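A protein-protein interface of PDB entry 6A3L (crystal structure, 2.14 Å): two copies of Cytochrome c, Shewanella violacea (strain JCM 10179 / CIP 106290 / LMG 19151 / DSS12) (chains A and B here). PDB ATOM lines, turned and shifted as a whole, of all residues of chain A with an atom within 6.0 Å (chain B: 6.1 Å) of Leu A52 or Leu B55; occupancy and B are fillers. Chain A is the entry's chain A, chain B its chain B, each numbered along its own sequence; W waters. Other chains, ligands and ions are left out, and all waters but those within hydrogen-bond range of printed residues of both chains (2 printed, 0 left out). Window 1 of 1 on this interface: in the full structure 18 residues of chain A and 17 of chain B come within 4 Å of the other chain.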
ATOM      1  N   SER A  15      14.716  12.113  -0.344  1.00  0.00           N
ATOM      2  CA  SER A  15      16.169  12.062  -0.486  1.00  0.00           C
ATOM      3  C   SER A  15      16.783  11.033   0.442  1.00  0.00           C
ATOM      4  O   SER A  15      17.751  10.359   0.072  1.00  0.00           O
ATOM      5  CB  SER A  15      16.798  13.428  -0.218  1.00  0.00           C
ATOM      6  OG  SER A  15      16.553  14.269  -1.312  1.00  0.00           O
ATOM      7  N   ALA A  16      16.290  10.952   1.675  1.00  0.00           N
ATOM      8  CA  ALA A  16      16.828   9.970   2.599  1.00  0.00           C
ATOM      9  C   ALA A  16      16.699   8.570   2.012  1.00  0.00           C
ATOM     10  O   ALA A  16      17.671   7.814   1.990  1.00  0.00           O
ATOM     11  CB  ALA A  16      16.132  10.091   3.954  1.00  0.00           C
ATOM     12  N   LEU A  19      19.082   8.118  -1.140  1.00  0.00           N
ATOM     13  CA  LEU A  19      20.448   7.848  -0.705  1.00  0.00           C
ATOM     14  C   LEU A  19      20.570   6.469  -0.074  1.00  0.00           C
ATOM     15  O   LEU A  19      21.637   5.842  -0.147  1.00  0.00           O
ATOM     16  CB  LEU A  19      20.903   8.909   0.291  1.00  0.00           C
ATOM     17  CG  LEU A  19      21.039  10.361  -0.216  1.00  0.00           C
ATOM     18  CD1 LEU A  19      21.617  11.256   0.857  1.00  0.00           C
ATOM     19  CD2 LEU A  19      21.937  10.417  -1.417  1.00  0.00           C
ATOM     20  N   MET A  20      19.504   5.996   0.581  1.00  0.00           N
ATOM     21  CA  MET A  20      19.526   4.670   1.187  1.00  0.00           C
ATOM     22  C   MET A  20      19.449   3.579   0.128  1.00  0.00           C
ATOM     23  O   MET A  20      20.131   2.552   0.242  1.00  0.00           O
ATOM     24  CB  MET A  20      18.385   4.552   2.197  1.00  0.00           C
ATOM     25  CG  MET A  20      18.316   3.228   2.918  1.00  0.00           C
ATOM     26  SD  MET A  20      17.382   3.441   4.448  1.00  0.00           S
ATOM     27  CE  MET A  20      15.713   3.680   3.854  1.00  0.00           C
ATOM     28  N   ALA A  21      18.625   3.779  -0.909  1.00  0.00           N
ATOM     29  CA  ALA A  21      18.534   2.793  -1.988  1.00  0.00           C
ATOM     30  C   ALA A  21      19.853   2.667  -2.737  1.00  0.00           C
ATOM     31  O   ALA A  21      20.246   1.555  -3.122  1.00  0.00           O
ATOM     32  CB  ALA A  21      17.424   3.158  -2.964  1.00  0.00           C
ATOM     33  N   ASN A  23      22.895   3.123  -1.555  1.00  0.00           N
ATOM     34  CA  ASN A  23      23.845   2.379  -0.740  1.00  0.00           C
ATOM     35  C   ASN A  23      23.422   0.924  -0.567  1.00  0.00           C
ATOM     36  O   ASN A  23      24.275   0.030  -0.555  1.00  0.00           O
ATOM     37  CB  ASN A  23      24.018   3.078   0.600  1.00  0.00           C
ATOM     38  CG  ASN A  23      24.872   4.325   0.475  1.00  0.00           C
ATOM     39  OD1 ASN A  23      26.090   4.270   0.636  1.00  0.00           O
ATOM     40  ND2 ASN A  23      24.238   5.445   0.124  1.00  0.00           N
ATOM     41  N   GLU A  47      27.221   0.945   7.061  1.00  0.00           N
ATOM     42  CA  GLU A  47      27.202   2.112   7.923  1.00  0.00           C
ATOM     43  C   GLU A  47      26.250   3.146   7.368  1.00  0.00           C
ATOM     44  O   GLU A  47      25.421   3.699   8.103  1.00  0.00           O
ATOM     45  CB  GLU A  47      28.617   2.680   8.045  1.00  0.00           C
ATOM     46  CG  GLU A  47      29.418   2.082   9.188  1.00  0.00           C
ATOM     47  CD  GLU A  47      30.859   2.552   9.210  1.00  0.00           C
ATOM     48  OE1 GLU A  47      31.216   3.418   8.387  1.00  0.00           O
ATOM     49  OE2 GLU A  47      31.638   2.036  10.041  1.00  0.00           O
ATOM     50  N   ASN A  48      26.314   3.373   6.053  1.00  0.00           N
ATOM     51  CA  ASN A  48      25.490   4.408   5.444  1.00  0.00           C
ATOM     52  C   ASN A  48      24.009   4.097   5.599  1.00  0.00           C
ATOM     53  O   ASN A  48      23.234   4.952   6.046  1.00  0.00           O
ATOM     54  CB  ASN A  48      25.874   4.596   3.973  1.00  0.00           C
ATOM     55  CG  ASN A  48      27.284   5.179   3.808  1.00  0.00           C
ATOM     56  OD1 ASN A  48      27.903   5.586   4.784  1.00  0.00           O
ATOM     57  ND2 ASN A  48      27.761   5.276   2.569  1.00  0.00           N
ATOM     58  N   VAL A  49      23.603   2.853   5.291  1.00  0.00           N
ATOM     59  CA  VAL A  49      22.174   2.526   5.323  1.00  0.00           C
ATOM     60  C   VAL A  49      21.641   2.659   6.741  1.00  0.00           C
ATOM     61  O   VAL A  49      20.551   3.195   6.967  1.00  0.00           O
ATOM     62  CB  VAL A  49      21.931   1.124   4.730  1.00  0.00           C
ATOM     63  CG1 VAL A  49      20.477   0.654   4.974  1.00  0.00           C
ATOM     64  CG2 VAL A  49      22.275   1.121   3.229  1.00  0.00           C
ATOM     65  N   ALA A  50      22.429   2.225   7.722  1.00  0.00           N
ATOM     66  CA  ALA A  50      22.022   2.336   9.119  1.00  0.00           C
ATOM     67  C   ALA A  50      21.777   3.790   9.511  1.00  0.00           C
ATOM     68  O   ALA A  50      20.738   4.125  10.101  1.00  0.00           O
ATOM     69  CB  ALA A  50      23.090   1.706  10.011  1.00  0.00           C
ATOM     70  N   ALA A  51      22.730   4.671   9.188  1.00  0.00           N
ATOM     71  CA  ALA A  51      22.556   6.083   9.506  1.00  0.00           C
ATOM     72  C   ALA A  51      21.410   6.683   8.702  1.00  0.00           C
ATOM     73  O   ALA A  51      20.596   7.438   9.243  1.00  0.00           O
ATOM     74  CB  ALA A  51      23.869   6.843   9.263  1.00  0.00           C
ATOM     75  N   LEU A  52      21.314   6.339   7.413  1.00  0.00           N
ATOM     76  CA  LEU A  52      20.240   6.878   6.584  1.00  0.00           C
ATOM     77  C   LEU A  52      18.869   6.437   7.078  1.00  0.00           C
ATOM     78  O   LEU A  52      17.901   7.204   6.995  1.00  0.00           O
ATOM     79  CB  LEU A  52      20.443   6.460   5.127  1.00  0.00           C
ATOM     80  CG  LEU A  52      21.535   7.288   4.404  1.00  0.00           C
ATOM     81  CD1 LEU A  52      22.014   6.627   3.097  1.00  0.00           C
ATOM     82  CD2 LEU A  52      21.089   8.742   4.156  1.00  0.00           C
ATOM     83  N   SER A  53      18.760   5.202   7.590  1.00  0.00           N
ATOM     84  CA  SER A  53      17.456   4.682   8.008  1.00  0.00           C
ATOM     85  C   SER A  53      16.857   5.488   9.156  1.00  0.00           C
ATOM     86  O   SER A  53      15.638   5.481   9.335  1.00  0.00           O
ATOM     87  CB  SER A  53      17.569   3.191   8.364  1.00  0.00           C
ATOM     88  OG  SER A  53      18.222   2.961   9.605  1.00  0.00           O
ATOM     89  N   LYS A  54      17.676   6.219   9.908  1.00  0.00           N
ATOM     90  CA  LYS A  54      17.194   7.062  11.000  1.00  0.00           C
ATOM     91  C   LYS A  54      16.602   8.415  10.549  1.00  0.00           C
ATOM     92  O   LYS A  54      16.040   9.137  11.385  1.00  0.00           O
ATOM     93  CB  LYS A  54      18.344   7.273  11.999  1.00  0.00           C
ATOM     94  CG  LYS A  54      18.835   5.955  12.575  1.00  0.00           C
ATOM     95  CD  LYS A  54      19.610   6.118  13.870  1.00  0.00           C
ATOM     96  CE  LYS A  54      21.113   5.910  13.661  1.00  0.00           C
ATOM     97  NZ  LYS A  54      21.814   5.413  14.889  1.00  0.00           N
ATOM     98  N   LEU A  55      16.719   8.799   9.268  1.00  0.00           N
ATOM     99  CA  LEU A  55      16.274  10.137   8.839  1.00  0.00           C
ATOM    100  C   LEU A  55      14.826  10.260   8.366  1.00  0.00           C
ATOM    101  O   LEU A  55      14.151  11.222   8.751  1.00  0.00           O
ATOM    102  CB  LEU A  55      17.171  10.681   7.724  1.00  0.00           C
ATOM    103  CG  LEU A  55      18.650  10.551   8.021  1.00  0.00           C
ATOM    104  CD1 LEU A  55      19.533  11.162   6.925  1.00  0.00           C
ATOM    105  CD2 LEU A  55      18.903  11.165   9.373  1.00  0.00           C
ATOM    106  N   PRO A  56      14.321   9.361   7.508  1.00  0.00           N
ATOM    107  CA  PRO A  56      13.062   9.673   6.801  1.00  0.00           C
ATOM    108  C   PRO A  56      11.840   9.795   7.695  1.00  0.00           C
ATOM    109  O   PRO A  56      10.885  10.482   7.306  1.00  0.00           O
ATOM    110  CB  PRO A  56      12.909   8.516   5.806  1.00  0.00           C
ATOM    111  CG  PRO A  56      13.750   7.428   6.327  1.00  0.00           C
ATOM    112  CD  PRO A  56      14.878   8.069   7.079  1.00  0.00           C
ATOM    113  N   TYR B  12      22.489  12.236  -6.247  1.00  0.00           N
ATOM    114  CA  TYR B  12      22.984  11.674  -5.002  1.00  0.00           C
ATOM    115  C   TYR B  12      23.638  12.748  -4.144  1.00  0.00           C
ATOM    116  O   TYR B  12      23.208  12.994  -3.011  1.00  0.00           O
ATOM    117  CB  TYR B  12      23.962  10.540  -5.297  1.00  0.00           C
ATOM    118  CG  TYR B  12      24.472   9.811  -4.078  1.00  0.00           C
ATOM    119  CD1 TYR B  12      23.857   8.646  -3.627  1.00  0.00           C
ATOM    120  CD2 TYR B  12      25.593  10.252  -3.399  1.00  0.00           C
ATOM    121  CE1 TYR B  12      24.354   7.957  -2.525  1.00  0.00           C
ATOM    122  CE2 TYR B  12      26.090   9.562  -2.284  1.00  0.00           C
ATOM    123  CZ  TYR B  12      25.471   8.415  -1.858  1.00  0.00           C
ATOM    124  OH  TYR B  12      25.961   7.730  -0.747  1.00  0.00           O
ATOM    125  N   ARG B  13      24.653  13.439  -4.686  1.00  0.00           N
ATOM    126  CA  ARG B  13      25.354  14.447  -3.884  1.00  0.00           C
ATOM    127  C   ARG B  13      24.434  15.593  -3.465  1.00  0.00           C
ATOM    128  O   ARG B  13      24.478  16.036  -2.308  1.00  0.00           O
ATOM    129  CB  ARG B  13      26.586  14.984  -4.632  1.00  0.00           C
ATOM    130  CG  ARG B  13      26.318  15.771  -5.895  1.00  0.00           C
ATOM    131  CD  ARG B  13      27.497  15.652  -6.865  1.00  0.00           C
ATOM    132  NE  ARG B  13      27.469  16.693  -7.896  1.00  0.00           N
ATOM    133  CZ  ARG B  13      28.028  16.576  -9.102  1.00  0.00           C
ATOM    134  NH1 ARG B  13      28.667  15.465  -9.456  1.00  0.00           N
ATOM    135  NH2 ARG B  13      27.947  17.570  -9.966  1.00  0.00           N
ATOM    136  N   ALA B  16      22.437  14.518  -0.457  1.00  0.00           N
ATOM    137  CA  ALA B  16      23.246  14.484   0.757  1.00  0.00           C
ATOM    138  C   ALA B  16      23.412  15.886   1.320  1.00  0.00           C
ATOM    139  O   ALA B  16      23.124  16.132   2.495  1.00  0.00           O
ATOM    140  CB  ALA B  16      24.609  13.841   0.484  1.00  0.00           C
ATOM    141  N   LEU B  19      20.057  17.172   2.971  1.00  0.00           N
ATOM    142  CA  LEU B  19      19.789  16.554   4.271  1.00  0.00           C
ATOM    143  C   LEU B  19      20.800  16.982   5.321  1.00  0.00           C
ATOM    144  O   LEU B  19      20.497  17.009   6.522  1.00  0.00           O
ATOM    145  CB  LEU B  19      19.808  15.024   4.146  1.00  0.00           C
ATOM    146  CG  LEU B  19      18.800  14.331   3.236  1.00  0.00           C
ATOM    147  CD1 LEU B  19      18.911  12.807   3.402  1.00  0.00           C
ATOM    148  CD2 LEU B  19      17.402  14.812   3.485  1.00  0.00           C
ATOM    149  N   ALA B  51      27.350  11.502   9.676  1.00  0.00           N
ATOM    150  CA  ALA B  51      27.120  10.449   8.688  1.00  0.00           C
ATOM    151  C   ALA B  51      26.818  11.033   7.318  1.00  0.00           C
ATOM    152  O   ALA B  51      27.334  10.544   6.305  1.00  0.00           O
ATOM    153  CB  ALA B  51      25.975   9.541   9.131  1.00  0.00           C
ATOM    154  N   LEU B  52      25.975  12.067   7.266  1.00  0.00           N
ATOM    155  CA  LEU B  52      25.639  12.671   5.979  1.00  0.00           C
ATOM    156  C   LEU B  52      26.864  13.279   5.307  1.00  0.00           C
ATOM    157  O   LEU B  52      27.012  13.196   4.083  1.00  0.00           O
ATOM    158  CB  LEU B  52      24.530  13.700   6.161  1.00  0.00           C
ATOM    159  CG  LEU B  52      23.135  13.064   6.232  1.00  0.00           C
ATOM    160  CD1 LEU B  52      22.076  14.004   6.821  1.00  0.00           C
ATOM    161  CD2 LEU B  52      22.750  12.677   4.831  1.00  0.00           C
ATOM    162  N   SER B  53      27.779  13.854   6.095  1.00  0.00           N
ATOM    163  CA  SER B  53      28.981  14.456   5.535  1.00  0.00           C
ATOM    164  C   SER B  53      29.890  13.458   4.819  1.00  0.00           C
ATOM    165  O   SER B  53      30.698  13.885   3.983  1.00  0.00           O
ATOM    166  CB  SER B  53      29.766  15.170   6.645  1.00  0.00           C
ATOM    167  OG  SER B  53      30.420  14.258   7.519  1.00  0.00           O
ATOM    168  N   LYS B  54      29.803  12.143   5.135  1.00  0.00           N
ATOM    169  CA  LYS B  54      30.606  11.105   4.466  1.00  0.00           C
ATOM    170  C   LYS B  54      30.064  10.671   3.103  1.00  0.00           C
ATOM    171  O   LYS B  54      30.737   9.895   2.408  1.00  0.00           O
ATOM    172  CB  LYS B  54      30.728   9.829   5.316  1.00  0.00           C
ATOM    173  CG  LYS B  54      31.417   9.929   6.684  1.00  0.00           C
ATOM    174  CD  LYS B  54      31.850   8.522   7.128  1.00  0.00           C
ATOM    175  CE  LYS B  54      31.528   8.247   8.582  1.00  0.00           C
ATOM    176  NZ  LYS B  54      30.685   7.005   8.762  1.00  0.00           N
ATOM    177  N   LEU B  55      28.866  11.098   2.717  1.00  0.00           N
ATOM    178  CA  LEU B  55      28.233  10.642   1.480  1.00  0.00           C
ATOM    179  C   LEU B  55      28.569  11.410   0.199  1.00  0.00           C
ATOM    180  O   LEU B  55      28.810  10.760  -0.832  1.00  0.00           O
ATOM    181  CB  LEU B  55      26.711  10.618   1.663  1.00  0.00           C
ATOM    182  CG  LEU B  55      26.285   9.873   2.937  1.00  0.00           C
ATOM    183  CD1 LEU B  55      24.785   9.822   3.079  1.00  0.00           C
ATOM    184  CD2 LEU B  55      26.873   8.473   2.880  1.00  0.00           C
ATOM    185  N   PRO B  56      28.575  12.762   0.190  1.00  0.00           N
ATOM    186  CA  PRO B  56      28.554  13.468  -1.108  1.00  0.00           C
ATOM    187  C   PRO B  56      29.793  13.282  -1.974  1.00  0.00           C
ATOM    188  O   PRO B  56      29.658  13.351  -3.203  1.00  0.00           O
ATOM    189  CB  PRO B  56      28.358  14.946  -0.719  1.00  0.00           C
ATOM    190  CG  PRO B  56      28.762  15.057   0.680  1.00  0.00           C
ATOM    191  CD  PRO B  56      28.506  13.709   1.322  1.00  0.00           C
ATOM    192  N   LEU B  57      30.980  13.041  -1.398  1.00  0.00           N
ATOM    193  CA  LEU B  57      32.190  12.990  -2.221  1.00  0.00           C
ATOM    194  C   LEU B  57      32.075  11.951  -3.334  1.00  0.00           C
ATOM    195  O   LEU B  57      32.520  12.192  -4.468  1.00  0.00           O
ATOM    196  CB  LEU B  57      33.426  12.694  -1.368  1.00  0.00           C
ATOM    197  CG  LEU B  57      34.782  12.793  -2.098  1.00  0.00           C
ATOM    198  CD1 LEU B  57      35.012  14.174  -2.699  1.00  0.00           C
ATOM    199  CD2 LEU B  57      35.944  12.399  -1.204  1.00  0.00           C
ATOM    200  N   GLU B  58      31.495  10.775  -3.018  1.00  0.00           N
ATOM    201  CA  GLU B  58      31.317   9.729  -4.015  1.00  0.00           C
ATOM    202  C   GLU B  58      30.615  10.267  -5.250  1.00  0.00           C
ATOM    203  O   GLU B  58      30.946   9.881  -6.378  1.00  0.00           O
ATOM    204  CB  GLU B  58      30.493   8.574  -3.403  1.00  0.00           C
ATOM    205  CG  GLU B  58      30.235   7.417  -4.325  1.00  0.00           C
ATOM    206  CD  GLU B  58      29.419   6.277  -3.678  1.00  0.00           C
ATOM    207  OE1 GLU B  58      29.174   6.280  -2.441  1.00  0.00           O
ATOM    208  OE2 GLU B  58      29.035   5.357  -4.433  1.00  0.00           O
ATOM    209  N   GLY B  59      29.698  11.214  -5.062  1.00  0.00           N
ATOM    210  CA  GLY B  59      28.932  11.792  -6.161  1.00  0.00           C
ATOM    211  C   GLY B  59      29.733  12.561  -7.204  1.00  0.00           C
ATOM    212  O   GLY B  59      29.256  12.721  -8.329  1.00  0.00           O
ATOM    213  N   GLN B  90      34.422  15.960   6.771  1.00  0.00           N
ATOM    214  CA  GLN B  90      34.093  14.736   7.495  1.00  0.00           C
ATOM    215  C   GLN B  90      34.747  14.753   8.864  1.00  0.00           C
ATOM    216  O   GLN B  90      34.097  14.481   9.877  1.00  0.00           O
ATOM    217  CB  GLN B  90      34.530  13.498   6.701  1.00  0.00           C
ATOM    218  CG  GLN B  90      33.902  13.420   5.322  1.00  0.00           C
ATOM    219  CD  GLN B  90      34.523  12.382   4.428  1.00  0.00           C
ATOM    220  OE1 GLN B  90      35.359  11.583   4.858  1.00  0.00           O
ATOM    221  NE2 GLN B  90      34.130  12.390   3.163  1.00  0.00           N
HETATM  222  O   HOH W   1      30.090   6.646   1.861  1.00  0.00           O
HETATM  223  O   HOH W   2      27.404   7.693   6.727  1.00  0.00           O
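The side-chain amide nitrogen (ND2) of Asn A23 is in hydrogen-bond range of the side-chain hydroxyl (OH) of Tyr B12 (3.0 Å).
OE1 of Glu A47 is in salt-bridge range of NZ of Lys B54 (3.6 Å).
ND2 of Asn A23 lies within hydrogen-bond range of O of Leu A19 (2.6 Å).
The side-chain amide nitrogen of Asn A48 sits at hydrogen-bond distance from the side-chain amide oxygen of Asn A23, at 2.7 Å.
Among the printed residues, pairs that only touch across the chains: Leu A19 with Tyr B12, Asn A48 with Leu B55, Ala A51 with Ala B51, Ala A16 with Leu B19, Leu A19 with Ala B16, Leu A55 with Leu B52, Leu A55 with Leu B19, Leu A52 with Leu B55 and Ser A15 with Leu B19.
Of the printed residues of chain B, Leu A52 touches Leu B55.
Printed residues of chain A within 4 Å of Leu B55: Asn A48 (3.3 Å) and Leu A52 (3.998 Å).
Of the printed residues of chain A, Tyr B12 touches Leu A19 and Asn A23.
Printed residues of chain A within 4 Å of Ala B51: Ala A51 (3.4 Å).
Ala A50 touches none of the printed residues of chain B.
The nearest printed residue of chain B that does not touch Leu A52 is Leu B52 (4.3 Å).
The nearest printed residue of chain A that does not touch Leu B52 is Leu A52 (4.3 Å).
Of the 14 printed residues of chain B, 7 touch a printed residue of chain A.
Printed residues of chain B that touch a printed residue of chain A: Tyr B12, Ala B16, Leu B19, Ala B51, Leu B52, Lys B54 and Leu B55.
Hydrophobic or aromatic side chains of chain B within 4 Å of the printed part of chain A: Tyr B12, Ala B16, Leu B19, Ala B51, Leu B52 and Leu B55.
Among the printed residues, Asp or Glu carboxylates within 4 Å of a Lys or Arg side-chain nitrogen of the other chain: Glu A47 with Lys B54 (3.6 Å).
Ala A16 touches Leu B19, and with the chains exchanged Leu A19 touches Ala B16.
Ala A51 touches its own counterpart, Ala B51.
Leu A52 touches Leu B55, and with the chains exchanged Leu A55 touches Leu B52.
Leu A55 touches Leu B19, but with the chains exchanged Leu A19 does not touch Leu B55 (4.1 Å).
Positions printed for both chains: 16, 19, 51, 52, 53, 54, 55 and 56.
Of the 11 pairs that touch across the chains among the printed residues, 5 have their exchanged pair printed and touching as well.
Water W1 lies within hydrogen-bond range of ND2 of Asn A48 and O of Lys B54.
Water W2 bridges O of Ala B51 (2.9 Å) and OD1 of Asn A48 (2.9 Å).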
